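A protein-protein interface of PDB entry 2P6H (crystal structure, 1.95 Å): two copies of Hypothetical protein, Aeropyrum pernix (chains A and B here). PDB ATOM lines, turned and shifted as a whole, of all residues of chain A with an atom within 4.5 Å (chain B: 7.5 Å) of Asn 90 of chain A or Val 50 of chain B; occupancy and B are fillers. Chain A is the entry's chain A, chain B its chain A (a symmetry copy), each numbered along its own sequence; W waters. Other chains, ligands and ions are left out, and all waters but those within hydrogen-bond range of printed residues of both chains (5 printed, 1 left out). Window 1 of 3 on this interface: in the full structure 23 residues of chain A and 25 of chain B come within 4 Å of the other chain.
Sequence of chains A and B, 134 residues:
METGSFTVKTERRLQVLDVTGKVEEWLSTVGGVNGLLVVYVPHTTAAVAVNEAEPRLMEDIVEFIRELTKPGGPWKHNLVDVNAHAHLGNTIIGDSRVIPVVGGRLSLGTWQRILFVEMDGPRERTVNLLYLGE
O of His 43 of chain A sits at hydrogen-bond distance from NE2 of Gln 112 of chain B (3.2 Å). The side-chain amide nitrogen (ND2) of Asn 51 of chain B is in hydrogen-bond range of the backbone carbonyl oxygen (O) of Thr 44 of chain A, 3.0 Å away. OD1 of Asn 51 of chain B lies within hydrogen-bond range of ND1 of His 87 of chain A (2.8 Å). The side-chain amide nitrogen (ND2) of Asn 90 of chain A is in hydrogen-bond range of the backbone carbonyl oxygen (O) of Val 50 of chain B (3.1 Å). The side-chain amide nitrogen of Asn 90 of chain A lies close to the side-chain amide nitrogen of Asn 51 of chain B. The side-chain carboxylate (OD1) of Asp 95 of chain A lies within salt-bridge range of the guanidinium group (NE) of Arg 97 of chain B, at 2.6 Å. O of Ile 92 of chain A sits close to O of Ile 92 of chain B (3.1 Å). OD2 of Asp 95 of chain A sits close to O of Val 50 of chain B (3.4 Å).
OD1 of Asn 90 of chain A sits close to O of His 43 of chain A (3.3 Å). The side-chain hydroxyl of Thr 44 of chain A lies close to a ring nitrogen (ND1) of His 87 of chain A (3.4 Å). O of Val 39 of chain B sits at hydrogen-bond distance from N of Arg 97 of chain B (2.8 Å). The backbone carbonyl oxygen of Asn 51 of chain B lies within hydrogen-bond range of the backbone NH of Arg 113 of chain B, at 2.8 Å.
Glu 52 of chain B touches Thr 44 of chain A. Thr 44 of chain A touches Gln 112 of chain B (CG2 to CG, 3.6 Å). CE1 of His 87 of chain A touches OE1 of Glu 52 of chain B (3.2 Å). CG1 of Ile 61 of chain B touches CD2 of Leu 88 of chain A, at 3.9 Å. Asn 51 of chain B touches Thr 91 of chain A (ND2 to CG2, 3.9 Å). Thr 91 of chain A touches Ile 93 of chain B. Phe 64 of chain B touches Ile 92 of chain A (CZ to CD1, 3.9 Å).
Asn 90 of chain A touches just these residues of chain B: Val 50 (3.1 Å) and Asn 51 (2.8 Å). Of the printed residues of chain A, Val 50 of chain B touches Asn 90 and Asp 95. Gly 89 of chain A touches none of the printed residues of chain B. Of the printed residues of chain B, His 87 of chain A touches Asn 51 (2.8 Å) and Glu 52 (3.2 Å). Printed residues of chain A within 4 Å of Ile 92 of chain B: Ile 92. Printed residues of chain A within 4 Å of Ile 93 of chain B: Thr 91 (3.9 Å). The nearest residue of chain B that does not touch Asn 90 of chain A is Gln 112 of chain B (5.2 Å). The nearest printed residue of chain A that does not touch Val 50 of chain B is Thr 91 of chain A (5.2 Å). The nearest printed residue of chain A that does not touch Arg 97 of chain B is Gly 94 of chain A (6.3 Å).
Hydrophobic or aromatic side chains of chain A that line the printed part of chain B: His 87, Leu 88 and Ile 92. Along chain A the printed residues that touch a printed residue of chain B span positions 43 to 95. Among the printed residues, 18 pairs touch across the chains. Among the printed residues, Asp or Glu carboxylates within 4 Å of a Lys or Arg side-chain nitrogen of the other chain: Asp 95 of chain A with Arg 97 of chain B (2.6 Å).
Ile 92 of chain B touches its own counterpart, Ile 92 of chain A. 2 positions are printed for both chains.
Water W1 lies within hydrogen-bond range of the side-chain amide nitrogen of Asn 90 of chain A (2.9 Å), the backbone carbonyl oxygen of Val 50 of chain B (3.0 Å) and the side-chain carboxylate of Asp 95 of chain A (3.3 Å). Water W2 lies within hydrogen-bond range of O of Ile 92 of chain B (3.2 Å) and O of Ile 92 of chain A (3.2 Å).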
ATOM      1  N   HIS A  43      29.119   6.263  21.896  1.00  0.00           N
ATOM      2  CA  HIS A  43      29.925   5.752  23.010  1.00  0.00           C
ATOM      3  C   HIS A  43      29.099   5.383  24.243  1.00  0.00           C
ATOM      4  O   HIS A  43      28.139   6.075  24.570  1.00  0.00           O
ATOM      5  CB  HIS A  43      30.982   6.791  23.407  1.00  0.00           C
ATOM      6  CG  HIS A  43      31.812   7.283  22.260  1.00  0.00           C
ATOM      7  ND1 HIS A  43      32.614   6.451  21.508  1.00  0.00           N
ATOM      8  CD2 HIS A  43      31.958   8.524  21.733  1.00  0.00           C
ATOM      9  CE1 HIS A  43      33.218   7.156  20.567  1.00  0.00           C
ATOM     10  NE2 HIS A  43      32.836   8.416  20.681  1.00  0.00           N
ATOM     11  N   THR A  44      29.483   4.295  24.910  1.00  0.00           N
ATOM     12  CA  THR A  44      28.808   3.851  26.127  1.00  0.00           C
ATOM     13  C   THR A  44      29.517   4.419  27.369  1.00  0.00           C
ATOM     14  O   THR A  44      29.034   4.251  28.483  1.00  0.00           O
ATOM     15  CB  THR A  44      28.812   2.307  26.270  1.00  0.00           C
ATOM     16  OG1 THR A  44      30.164   1.843  26.398  1.00  0.00           O
ATOM     17  CG2 THR A  44      28.154   1.640  25.067  1.00  0.00           C
ATOM     18  N   ALA A  46      30.750   7.757  27.356  1.00  0.00           N
ATOM     19  CA  ALA A  46      30.731   9.199  27.170  1.00  0.00           C
ATOM     20  C   ALA A  46      29.285   9.552  26.985  1.00  0.00           C
ATOM     21  O   ALA A  46      28.443   8.706  26.711  1.00  0.00           O
ATOM     22  CB  ALA A  46      31.595   9.670  25.940  1.00  0.00           C
ATOM     23  N   ALA A  47      28.942  10.821  27.164  1.00  0.00           N
ATOM     24  CA  ALA A  47      27.547  11.231  27.026  1.00  0.00           C
ATOM     25  C   ALA A  47      27.456  12.641  26.456  1.00  0.00           C
ATOM     26  O   ALA A  47      28.462  13.288  26.188  1.00  0.00           O
ATOM     27  CB  ALA A  47      26.869  11.181  28.403  1.00  0.00           C
ATOM     28  N   ALA A  86      32.003   5.272  34.142  1.00  0.00           N
ATOM     29  CA  ALA A  86      31.644   5.983  32.912  1.00  0.00           C
ATOM     30  C   ALA A  86      30.340   5.442  32.319  1.00  0.00           C
ATOM     31  O   ALA A  86      29.492   6.181  31.837  1.00  0.00           O
ATOM     32  CB  ALA A  86      32.791   5.854  31.889  1.00  0.00           C
ATOM     33  N   HIS A  87      30.170   4.123  32.341  1.00  0.00           N
ATOM     34  CA  HIS A  87      28.952   3.509  31.828  1.00  0.00           C
ATOM     35  C   HIS A  87      27.774   4.017  32.662  1.00  0.00           C
ATOM     36  O   HIS A  87      26.731   4.380  32.126  1.00  0.00           O
ATOM     37  CB  HIS A  87      29.042   1.979  31.935  1.00  0.00           C
ATOM     38  CG  HIS A  87      30.084   1.360  31.047  1.00  0.00           C
ATOM     39  ND1 HIS A  87      29.841   1.026  29.732  1.00  0.00           N
ATOM     40  CD2 HIS A  87      31.359   0.976  31.304  1.00  0.00           C
ATOM     41  CE1 HIS A  87      30.920   0.452  29.219  1.00  0.00           C
ATOM     42  NE2 HIS A  87      31.852   0.409  30.151  1.00  0.00           N
ATOM     43  N   LEU A  88      27.962   4.052  33.979  1.00  0.00           N
ATOM     44  CA  LEU A  88      26.925   4.507  34.893  1.00  0.00           C
ATOM     45  C   LEU A  88      26.561   5.974  34.621  1.00  0.00           C
ATOM     46  O   LEU A  88      25.381   6.333  34.587  1.00  0.00           O
ATOM     47  CB  LEU A  88      27.393   4.325  36.343  1.00  0.00           C
ATOM     48  CG  LEU A  88      27.750   2.887  36.753  1.00  0.00           C
ATOM     49  CD1 LEU A  88      28.187   2.879  38.203  1.00  0.00           C
ATOM     50  CD2 LEU A  88      26.553   1.949  36.548  1.00  0.00           C
ATOM     51  N   GLY A  89      27.566   6.818  34.414  1.00  0.00           N
ATOM     52  CA  GLY A  89      27.287   8.218  34.129  1.00  0.00           C
ATOM     53  C   GLY A  89      26.491   8.356  32.840  1.00  0.00           C
ATOM     54  O   GLY A  89      25.523   9.129  32.750  1.00  0.00           O
ATOM     55  N   ASN A  90      26.905   7.600  31.828  1.00  0.00           N
ATOM     56  CA  ASN A  90      26.217   7.613  30.542  1.00  0.00           C
ATOM     57  C   ASN A  90      24.748   7.252  30.690  1.00  0.00           C
ATOM     58  O   ASN A  90      23.891   7.826  30.058  1.00  0.00           O
ATOM     59  CB  ASN A  90      26.905   6.638  29.572  1.00  0.00           C
ATOM     60  CG  ASN A  90      26.086   6.413  28.309  1.00  0.00           C
ATOM     61  OD1 ASN A  90      26.426   6.871  27.228  1.00  0.00           O
ATOM     62  ND2 ASN A  90      24.983   5.658  28.454  1.00  0.00           N
ATOM     63  N   THR A  91      24.440   6.237  31.553  1.00  0.00           N
ATOM     64  CA  THR A  91      23.024   5.860  31.669  1.00  0.00           C
ATOM     65  C   THR A  91      22.124   6.962  32.247  1.00  0.00           C
ATOM     66  O   THR A  91      20.945   7.025  31.950  1.00  0.00           O
ATOM     67  CB  THR A  91      22.825   4.557  32.483  1.00  0.00           C
ATOM     68  OG1 THR A  91      22.900   4.834  33.885  1.00  0.00           O
ATOM     69  CG2 THR A  91      23.832   3.473  32.113  1.00  0.00           C
ATOM     70  N   ILE A  92      22.632   7.816  33.166  1.00  0.00           N
ATOM     71  CA  ILE A  92      21.628   8.809  33.659  1.00  0.00           C
ATOM     72  C   ILE A  92      21.858  10.185  33.070  1.00  0.00           C
ATOM     73  O   ILE A  92      21.186  11.146  33.420  1.00  0.00           O
ATOM     74  CB  ILE A  92      21.763   9.000  35.150  1.00  0.00           C
ATOM     75  CG1 ILE A  92      23.244   9.280  35.475  1.00  0.00           C
ATOM     76  CG2 ILE A  92      21.316   7.715  35.877  1.00  0.00           C
ATOM     77  CD1 ILE A  92      23.569   9.730  36.901  1.00  0.00           C
ATOM     78  N   ILE A  93      22.855  10.321  32.158  1.00  0.00           N
ATOM     79  CA  ILE A  93      22.967  11.593  31.456  1.00  0.00           C
ATOM     80  C   ILE A  93      22.361  11.460  30.072  1.00  0.00           C
ATOM     81  O   ILE A  93      21.640  12.325  29.595  1.00  0.00           O
ATOM     82  CB  ILE A  93      24.452  11.998  31.336  1.00  0.00           C
ATOM     83  CG1 ILE A  93      25.013  12.418  32.696  1.00  0.00           C
ATOM     84  CG2 ILE A  93      24.604  13.190  30.376  1.00  0.00           C
ATOM     85  CD1 ILE A  93      26.540  12.547  32.677  1.00  0.00           C
ATOM     86  N   GLY A  94      22.603  10.334  29.405  1.00  0.00           N
ATOM     87  CA  GLY A  94      22.022  10.128  28.087  1.00  0.00           C
ATOM     88  C   GLY A  94      23.030  10.295  26.958  1.00  0.00           C
ATOM     89  O   GLY A  94      24.003  11.032  27.089  1.00  0.00           O
ATOM     90  N   ASP A  95      22.795   9.619  25.839  1.00  0.00           N
ATOM     91  CA  ASP A  95      23.719   9.681  24.713  1.00  0.00           C
ATOM     92  C   ASP A  95      23.165  10.361  23.468  1.00  0.00           C
ATOM     93  O   ASP A  95      23.802  10.339  22.414  1.00  0.00           O
ATOM     94  CB  ASP A  95      24.192   8.272  24.352  1.00  0.00           C
ATOM     95  CG  ASP A  95      23.070   7.272  24.377  1.00  0.00           C
ATOM     96  OD1 ASP A  95      21.915   7.678  24.135  1.00  0.00           O
ATOM     97  OD2 ASP A  95      23.339   6.083  24.635  1.00  0.00           O
ATOM     98  N   MET A 119      33.939  10.554  30.134  1.00  0.00           N
ATOM     99  CA  MET A 119      34.103   9.926  31.437  1.00  0.00           C
ATOM    100  C   MET A 119      35.171   8.834  31.420  1.00  0.00           C
ATOM    101  O   MET A 119      35.466   8.223  32.452  1.00  0.00           O
ATOM    102  CB  MET A 119      32.755   9.384  31.930  1.00  0.00           C
ATOM    103  CG  MET A 119      31.775  10.520  32.229  1.00  0.00           C
ATOM    104  SD  MET A 119      30.090  10.034  32.591  1.00  0.00           S
ATOM    105  CE  MET A 119      29.401   9.949  30.939  1.00  0.00           C
ATOM    106  N   VAL B  39      12.249   4.416  20.596  1.00  0.00           N
ATOM    107  CA  VAL B  39      12.010   3.341  21.523  1.00  0.00           C
ATOM    108  C   VAL B  39      11.546   3.955  22.798  1.00  0.00           C
ATOM    109  O   VAL B  39      12.213   4.790  23.396  1.00  0.00           O
ATOM    110  CB  VAL B  39      13.314   2.592  21.800  1.00  0.00           C
ATOM    111  CG1 VAL B  39      13.038   1.383  22.691  1.00  0.00           C
ATOM    112  CG2 VAL B  39      13.928   2.124  20.494  1.00  0.00           C
ATOM    113  N   VAL B  48      14.305   2.982  29.921  1.00  0.00           N
ATOM    114  CA  VAL B  48      15.154   2.412  28.881  1.00  0.00           C
ATOM    115  C   VAL B  48      16.402   3.240  28.755  1.00  0.00           C
ATOM    116  O   VAL B  48      16.381   4.460  28.828  1.00  0.00           O
ATOM    117  CB  VAL B  48      14.450   2.421  27.518  1.00  0.00           C
ATOM    118  CG1 VAL B  48      13.816   3.785  27.262  1.00  0.00           C
ATOM    119  CG2 VAL B  48      15.472   2.151  26.420  1.00  0.00           C
ATOM    120  N   ALA B  49      17.512   2.516  28.607  1.00  0.00           N
ATOM    121  CA  ALA B  49      18.788   3.160  28.472  1.00  0.00           C
ATOM    122  C   ALA B  49      19.567   2.520  27.348  1.00  0.00           C
ATOM    123  O   ALA B  49      19.238   1.444  26.866  1.00  0.00           O
ATOM    124  CB  ALA B  49      19.530   2.939  29.771  1.00  0.00           C
ATOM    125  N   VAL B  50      20.638   3.172  26.941  1.00  0.00           N
ATOM    126  CA  VAL B  50      21.516   2.600  25.934  1.00  0.00           C
ATOM    127  C   VAL B  50      22.902   2.499  26.478  1.00  0.00           C
ATOM    128  O   VAL B  50      23.514   3.480  26.881  1.00  0.00           O
ATOM    129  CB  VAL B  50      21.597   3.527  24.740  1.00  0.00           C
ATOM    130  CG1 VAL B  50      22.637   3.006  23.750  1.00  0.00           C
ATOM    131  CG2 VAL B  50      20.245   3.602  24.053  1.00  0.00           C
ATOM    132  N   ASN B  51      23.403   1.271  26.548  1.00  0.00           N
ATOM    133  CA  ASN B  51      24.769   1.056  27.008  1.00  0.00           C
ATOM    134  C   ASN B  51      25.193  -0.377  26.713  1.00  0.00           C
ATOM    135  O   ASN B  51      24.577  -1.084  25.925  1.00  0.00           O
ATOM    136  CB  ASN B  51      24.827   1.329  28.521  1.00  0.00           C
ATOM    137  CG  ASN B  51      26.179   1.897  28.915  1.00  0.00           C
ATOM    138  OD1 ASN B  51      27.146   1.173  29.137  1.00  0.00           O
ATOM    139  ND2 ASN B  51      26.228   3.236  29.008  1.00  0.00           N
ATOM    140  N   GLU B  52      26.298  -0.805  27.314  1.00  0.00           N
ATOM    141  CA  GLU B  52      26.867  -2.126  27.048  1.00  0.00           C
ATOM    142  C   GLU B  52      26.163  -3.249  27.801  1.00  0.00           C
ATOM    143  O   GLU B  52      25.926  -3.150  29.012  1.00  0.00           O
ATOM    144  CB  GLU B  52      28.362  -2.129  27.398  1.00  0.00           C
ATOM    145  CG  GLU B  52      29.139  -3.260  26.753  1.00  0.00           C
ATOM    146  CD  GLU B  52      30.651  -3.181  27.000  1.00  0.00           C
ATOM    147  OE1 GLU B  52      31.187  -2.063  27.239  1.00  0.00           O
ATOM    148  OE2 GLU B  52      31.307  -4.246  26.934  1.00  0.00           O
ATOM    149  N   ALA B  53      25.835  -4.322  27.084  1.00  0.00           N
ATOM    150  CA  ALA B  53      25.149  -5.459  27.699  1.00  0.00           C
ATOM    151  C   ALA B  53      26.151  -6.476  28.281  1.00  0.00           C
ATOM    152  O   ALA B  53      26.087  -7.670  28.019  1.00  0.00           O
ATOM    153  CB  ALA B  53      24.216  -6.112  26.650  1.00  0.00           C
ATOM    154  N   ILE B  61      24.635  -1.701  37.234  1.00  0.00           N
ATOM    155  CA  ILE B  61      23.609  -0.707  36.997  1.00  0.00           C
ATOM    156  C   ILE B  61      22.476  -0.817  38.011  1.00  0.00           C
ATOM    157  O   ILE B  61      21.968   0.165  38.536  1.00  0.00           O
ATOM    158  CB  ILE B  61      23.110  -0.934  35.586  1.00  0.00           C
ATOM    159  CG1 ILE B  61      24.209  -0.467  34.611  1.00  0.00           C
ATOM    160  CG2 ILE B  61      21.825  -0.095  35.381  1.00  0.00           C
ATOM    161  CD1 ILE B  61      23.899  -0.554  33.112  1.00  0.00           C
ATOM    162  N   PHE B  64      23.776   0.491  41.293  1.00  0.00           N
ATOM    163  CA  PHE B  64      23.919   1.944  41.203  1.00  0.00           C
ATOM    164  C   PHE B  64      22.562   2.593  41.455  1.00  0.00           C
ATOM    165  O   PHE B  64      22.415   3.536  42.209  1.00  0.00           O
ATOM    166  CB  PHE B  64      24.451   2.287  39.797  1.00  0.00           C
ATOM    167  CG  PHE B  64      24.501   3.779  39.505  1.00  0.00           C
ATOM    168  CD1 PHE B  64      25.312   4.620  40.256  1.00  0.00           C
ATOM    169  CD2 PHE B  64      23.791   4.282  38.424  1.00  0.00           C
ATOM    170  CE1 PHE B  64      25.405   5.971  39.921  1.00  0.00           C
ATOM    171  CE2 PHE B  64      23.888   5.636  38.094  1.00  0.00           C
ATOM    172  CZ  PHE B  64      24.696   6.482  38.839  1.00  0.00           C
ATOM    173  N   ILE B  92      15.571   9.908  36.209  1.00  0.00           N
ATOM    174  CA  ILE B  92      16.902  10.375  35.713  1.00  0.00           C
ATOM    175  C   ILE B  92      17.511   9.400  34.727  1.00  0.00           C
ATOM    176  O   ILE B  92      18.635   9.572  34.277  1.00  0.00           O
ATOM    177  CB  ILE B  92      17.893  10.447  36.848  1.00  0.00           C
ATOM    178  CG1 ILE B  92      17.858   9.107  37.611  1.00  0.00           C
ATOM    179  CG2 ILE B  92      17.497  11.588  37.807  1.00  0.00           C
ATOM    180  CD1 ILE B  92      18.948   8.878  38.661  1.00  0.00           C
ATOM    181  N   ILE B  93      16.775   8.312  34.382  1.00  0.00           N
ATOM    182  CA  ILE B  93      17.275   7.466  33.305  1.00  0.00           C
ATOM    183  C   ILE B  93      16.530   7.789  32.025  1.00  0.00           C
ATOM    184  O   ILE B  93      17.104   7.893  30.950  1.00  0.00           O
ATOM    185  CB  ILE B  93      17.067   5.980  33.666  1.00  0.00           C
ATOM    186  CG1 ILE B  93      18.026   5.551  34.780  1.00  0.00           C
ATOM    187  CG2 ILE B  93      17.342   5.090  32.441  1.00  0.00           C
ATOM    188  CD1 ILE B  93      17.660   4.181  35.362  1.00  0.00           C
ATOM    189  N   ARG B  97      14.052   6.817  23.864  1.00  0.00           N
ATOM    190  CA  ARG B  97      15.329   7.042  23.185  1.00  0.00           C
ATOM    191  C   ARG B  97      15.104   7.160  21.692  1.00  0.00           C
ATOM    192  O   ARG B  97      14.364   6.393  21.090  1.00  0.00           O
ATOM    193  CB  ARG B  97      16.257   5.851  23.485  1.00  0.00           C
ATOM    194  CG  ARG B  97      17.503   5.808  22.577  1.00  0.00           C
ATOM    195  CD  ARG B  97      18.405   7.050  22.725  1.00  0.00           C
ATOM    196  NE  ARG B  97      19.820   6.669  22.920  1.00  0.00           N
ATOM    197  CZ  ARG B  97      20.617   6.417  21.840  1.00  0.00           C
ATOM    198  NH1 ARG B  97      20.160   6.525  20.594  1.00  0.00           N
ATOM    199  NH2 ARG B  97      21.872   6.026  22.051  1.00  0.00           N
ATOM    200  N   VAL B  98      15.748   8.148  21.091  1.00  0.00           N
ATOM    201  CA  VAL B  98      15.644   8.316  19.650  1.00  0.00           C
ATOM    202  C   VAL B  98      16.924   7.764  19.054  1.00  0.00           C
ATOM    203  O   VAL B  98      18.012   8.072  19.492  1.00  0.00           O
ATOM    204  CB  VAL B  98      15.502   9.814  19.295  1.00  0.00           C
ATOM    205  CG1 VAL B  98      15.459   9.958  17.768  1.00  0.00           C
ATOM    206  CG2 VAL B  98      14.233  10.402  19.888  1.00  0.00           C
ATOM    207  N   ILE B  99      16.746   6.866  18.048  1.00  0.00           N
ATOM    208  CA  ILE B  99      17.891   6.222  17.388  1.00  0.00           C
ATOM    209  C   ILE B  99      17.792   6.352  15.877  1.00  0.00           C
ATOM    210  O   ILE B  99      16.904   5.807  15.233  1.00  0.00           O
ATOM    211  CB  ILE B  99      17.920   4.728  17.737  1.00  0.00           C
ATOM    212  CG1 ILE B  99      17.856   4.544  19.250  1.00  0.00           C
ATOM    213  CG2 ILE B  99      19.249   4.111  17.243  1.00  0.00           C
ATOM    214  CD1 ILE B  99      17.712   3.078  19.660  1.00  0.00           C
ATOM    215  N   LEU B 108      23.502   2.556  16.179  1.00  0.00           N
ATOM    216  CA  LEU B 108      24.007   2.340  17.530  1.00  0.00           C
ATOM    217  C   LEU B 108      25.505   2.137  17.404  1.00  0.00           C
ATOM    218  O   LEU B 108      25.990   1.672  16.363  1.00  0.00           O
ATOM    219  CB  LEU B 108      23.376   1.098  18.166  1.00  0.00           C
ATOM    220  CG  LEU B 108      21.907   1.221  18.568  1.00  0.00           C
ATOM    221  CD1 LEU B 108      21.398  -0.113  19.106  1.00  0.00           C
ATOM    222  CD2 LEU B 108      21.764   2.318  19.615  1.00  0.00           C
ATOM    223  N   GLY B 109      26.236   2.496  18.451  1.00  0.00           N
ATOM    224  CA  GLY B 109      27.677   2.334  18.433  1.00  0.00           C
ATOM    225  C   GLY B 109      28.048   0.872  18.535  1.00  0.00           C
ATOM    226  O   GLY B 109      27.199   0.023  18.784  1.00  0.00           O
ATOM    227  N   TRP B 111      29.474  -0.915  20.838  1.00  0.00           N
ATOM    228  CA  TRP B 111      29.124  -1.558  22.106  1.00  0.00           C
ATOM    229  C   TRP B 111      27.807  -1.106  22.729  1.00  0.00           C
ATOM    230  O   TRP B 111      27.502  -1.471  23.864  1.00  0.00           O
ATOM    231  CB  TRP B 111      30.264  -1.340  23.106  1.00  0.00           C
ATOM    232  CG  TRP B 111      31.610  -1.508  22.464  1.00  0.00           C
ATOM    233  CD1 TRP B 111      32.514  -0.528  22.180  1.00  0.00           C
ATOM    234  CD2 TRP B 111      32.144  -2.718  21.922  1.00  0.00           C
ATOM    235  NE1 TRP B 111      33.578  -1.048  21.484  1.00  0.00           N
ATOM    236  CE2 TRP B 111      33.375  -2.393  21.312  1.00  0.00           C
ATOM    237  CE3 TRP B 111      31.696  -4.045  21.887  1.00  0.00           C
ATOM    238  CZ2 TRP B 111      34.170  -3.351  20.671  1.00  0.00           C
ATOM    239  CZ3 TRP B 111      32.490  -5.000  21.246  1.00  0.00           C
ATOM    240  CH2 TRP B 111      33.713  -4.643  20.648  1.00  0.00           C
ATOM    241  N   GLN B 112      27.028  -0.312  21.996  1.00  0.00           N
ATOM    242  CA  GLN B 112      25.743   0.169  22.506  1.00  0.00           C
ATOM    243  C   GLN B 112      24.622  -0.828  22.265  1.00  0.00           C
ATOM    244  O   GLN B 112      24.510  -1.414  21.187  1.00  0.00           O
ATOM    245  CB  GLN B 112      25.359   1.504  21.855  1.00  0.00           C
ATOM    246  CG  GLN B 112      26.292   2.661  22.197  1.00  0.00           C
ATOM    247  CD  GLN B 112      25.821   3.992  21.622  1.00  0.00           C
ATOM    248  OE1 GLN B 112      25.358   4.066  20.481  1.00  0.00           O
ATOM    249  NE2 GLN B 112      25.950   5.053  22.414  1.00  0.00           N
ATOM    250  N   ARG B 113      23.784  -1.010  23.280  1.00  0.00           N
ATOM    251  CA  ARG B 113      22.651  -1.894  23.189  1.00  0.00           C
ATOM    252  C   ARG B 113      21.463  -1.250  23.870  1.00  0.00           C
ATOM    253  O   ARG B 113      21.599  -0.384  24.725  1.00  0.00           O
ATOM    254  CB  ARG B 113      23.009  -3.205  23.891  1.00  0.00           C
ATOM    255  CG  ARG B 113      24.206  -3.904  23.243  1.00  0.00           C
ATOM    256  CD  ARG B 113      23.770  -4.904  22.167  1.00  0.00           C
ATOM    257  NE  ARG B 113      24.937  -5.545  21.553  1.00  0.00           N
ATOM    258  CZ  ARG B 113      25.009  -6.887  21.616  1.00  0.00           C
ATOM    259  NH1 ARG B 113      24.052  -7.576  22.213  1.00  0.00           N
ATOM    260  NH2 ARG B 113      26.051  -7.520  21.070  1.00  0.00           N
ATOM    261  N   ILE B 114      20.260  -1.657  23.490  1.00  0.00           N
ATOM    262  CA  ILE B 114      19.033  -1.118  24.058  1.00  0.00           C
ATOM    263  C   ILE B 114      18.681  -1.906  25.292  1.00  0.00           C
ATOM    264  O   ILE B 114      18.338  -3.080  25.235  1.00  0.00           O
ATOM    265  CB  ILE B 114      17.876  -1.216  23.043  1.00  0.00           C
ATOM    266  CG1 ILE B 114      18.258  -0.487  21.753  1.00  0.00           C
ATOM    267  CG2 ILE B 114      16.622  -0.529  23.620  1.00  0.00           C
ATOM    268  CD1 ILE B 114      17.401  -0.664  20.500  1.00  0.00           C
ATOM    269  N   LEU B 115      18.746  -1.255  26.444  1.00  0.00           N
ATOM    270  CA  LEU B 115      18.488  -1.942  27.697  1.00  0.00           C
ATOM    271  C   LEU B 115      17.197  -1.534  28.392  1.00  0.00           C
ATOM    272  O   LEU B 115      16.955  -0.352  28.632  1.00  0.00           O
ATOM    273  CB  LEU B 115      19.656  -1.698  28.661  1.00  0.00           C
ATOM    274  CG  LEU B 115      21.041  -2.002  28.070  1.00  0.00           C
ATOM    275  CD1 LEU B 115      22.127  -1.625  29.048  1.00  0.00           C
ATOM    276  CD2 LEU B 115      21.131  -3.484  27.720  1.00  0.00           C
ATOM    277  N   PHE B 116      16.368  -2.522  28.709  1.00  0.00           N
ATOM    278  CA  PHE B 116      15.134  -2.273  29.438  1.00  0.00           C
ATOM    279  C   PHE B 116      15.569  -2.298  30.900  1.00  0.00           C
ATOM    280  O   PHE B 116      16.230  -3.243  31.344  1.00  0.00           O
ATOM    281  CB  PHE B 116      14.109  -3.384  29.211  1.00  0.00           C
ATOM    282  CG  PHE B 116      12.778  -3.104  29.852  1.00  0.00           C
ATOM    283  CD1 PHE B 116      12.561  -3.405  31.190  1.00  0.00           C
ATOM    284  CD2 PHE B 116      11.746  -2.513  29.123  1.00  0.00           C
ATOM    285  CE1 PHE B 116      11.341  -3.124  31.800  1.00  0.00           C
ATOM    286  CE2 PHE B 116      10.516  -2.227  29.721  1.00  0.00           C
ATOM    287  CZ  PHE B 116      10.314  -2.534  31.062  1.00  0.00           C
ATOM    288  N   VAL B 117      15.210  -1.260  31.641  1.00  0.00           N
ATOM    289  CA  VAL B 117      15.567  -1.194  33.045  1.00  0.00           C
ATOM    290  C   VAL B 117      14.338  -1.321  33.919  1.00  0.00           C
ATOM    291  O   VAL B 117      13.551  -0.397  34.070  1.00  0.00           O
ATOM    292  CB  VAL B 117      16.188   0.162  33.301  1.00  0.00           C
ATOM    293  CG1 VAL B 117      16.657   0.255  34.752  1.00  0.00           C
ATOM    294  CG2 VAL B 117      17.371   0.376  32.376  1.00  0.00           C
HETATM  295  O   HOH W   1      22.230   6.073  27.786  1.00  0.00           O
HETATM  296  O   HOH W   2      18.517  11.389  31.594  1.00  0.00           O
HETATM  297  O   HOH W   3      19.508   9.399  30.453  1.00  0.00           O
HETATM  298  O   HOH W   4      20.395   6.861  25.954  1.00  0.00           O
HETATM  299  O   HOH W   5      33.582  -1.684  28.804  1.00  0.00           O
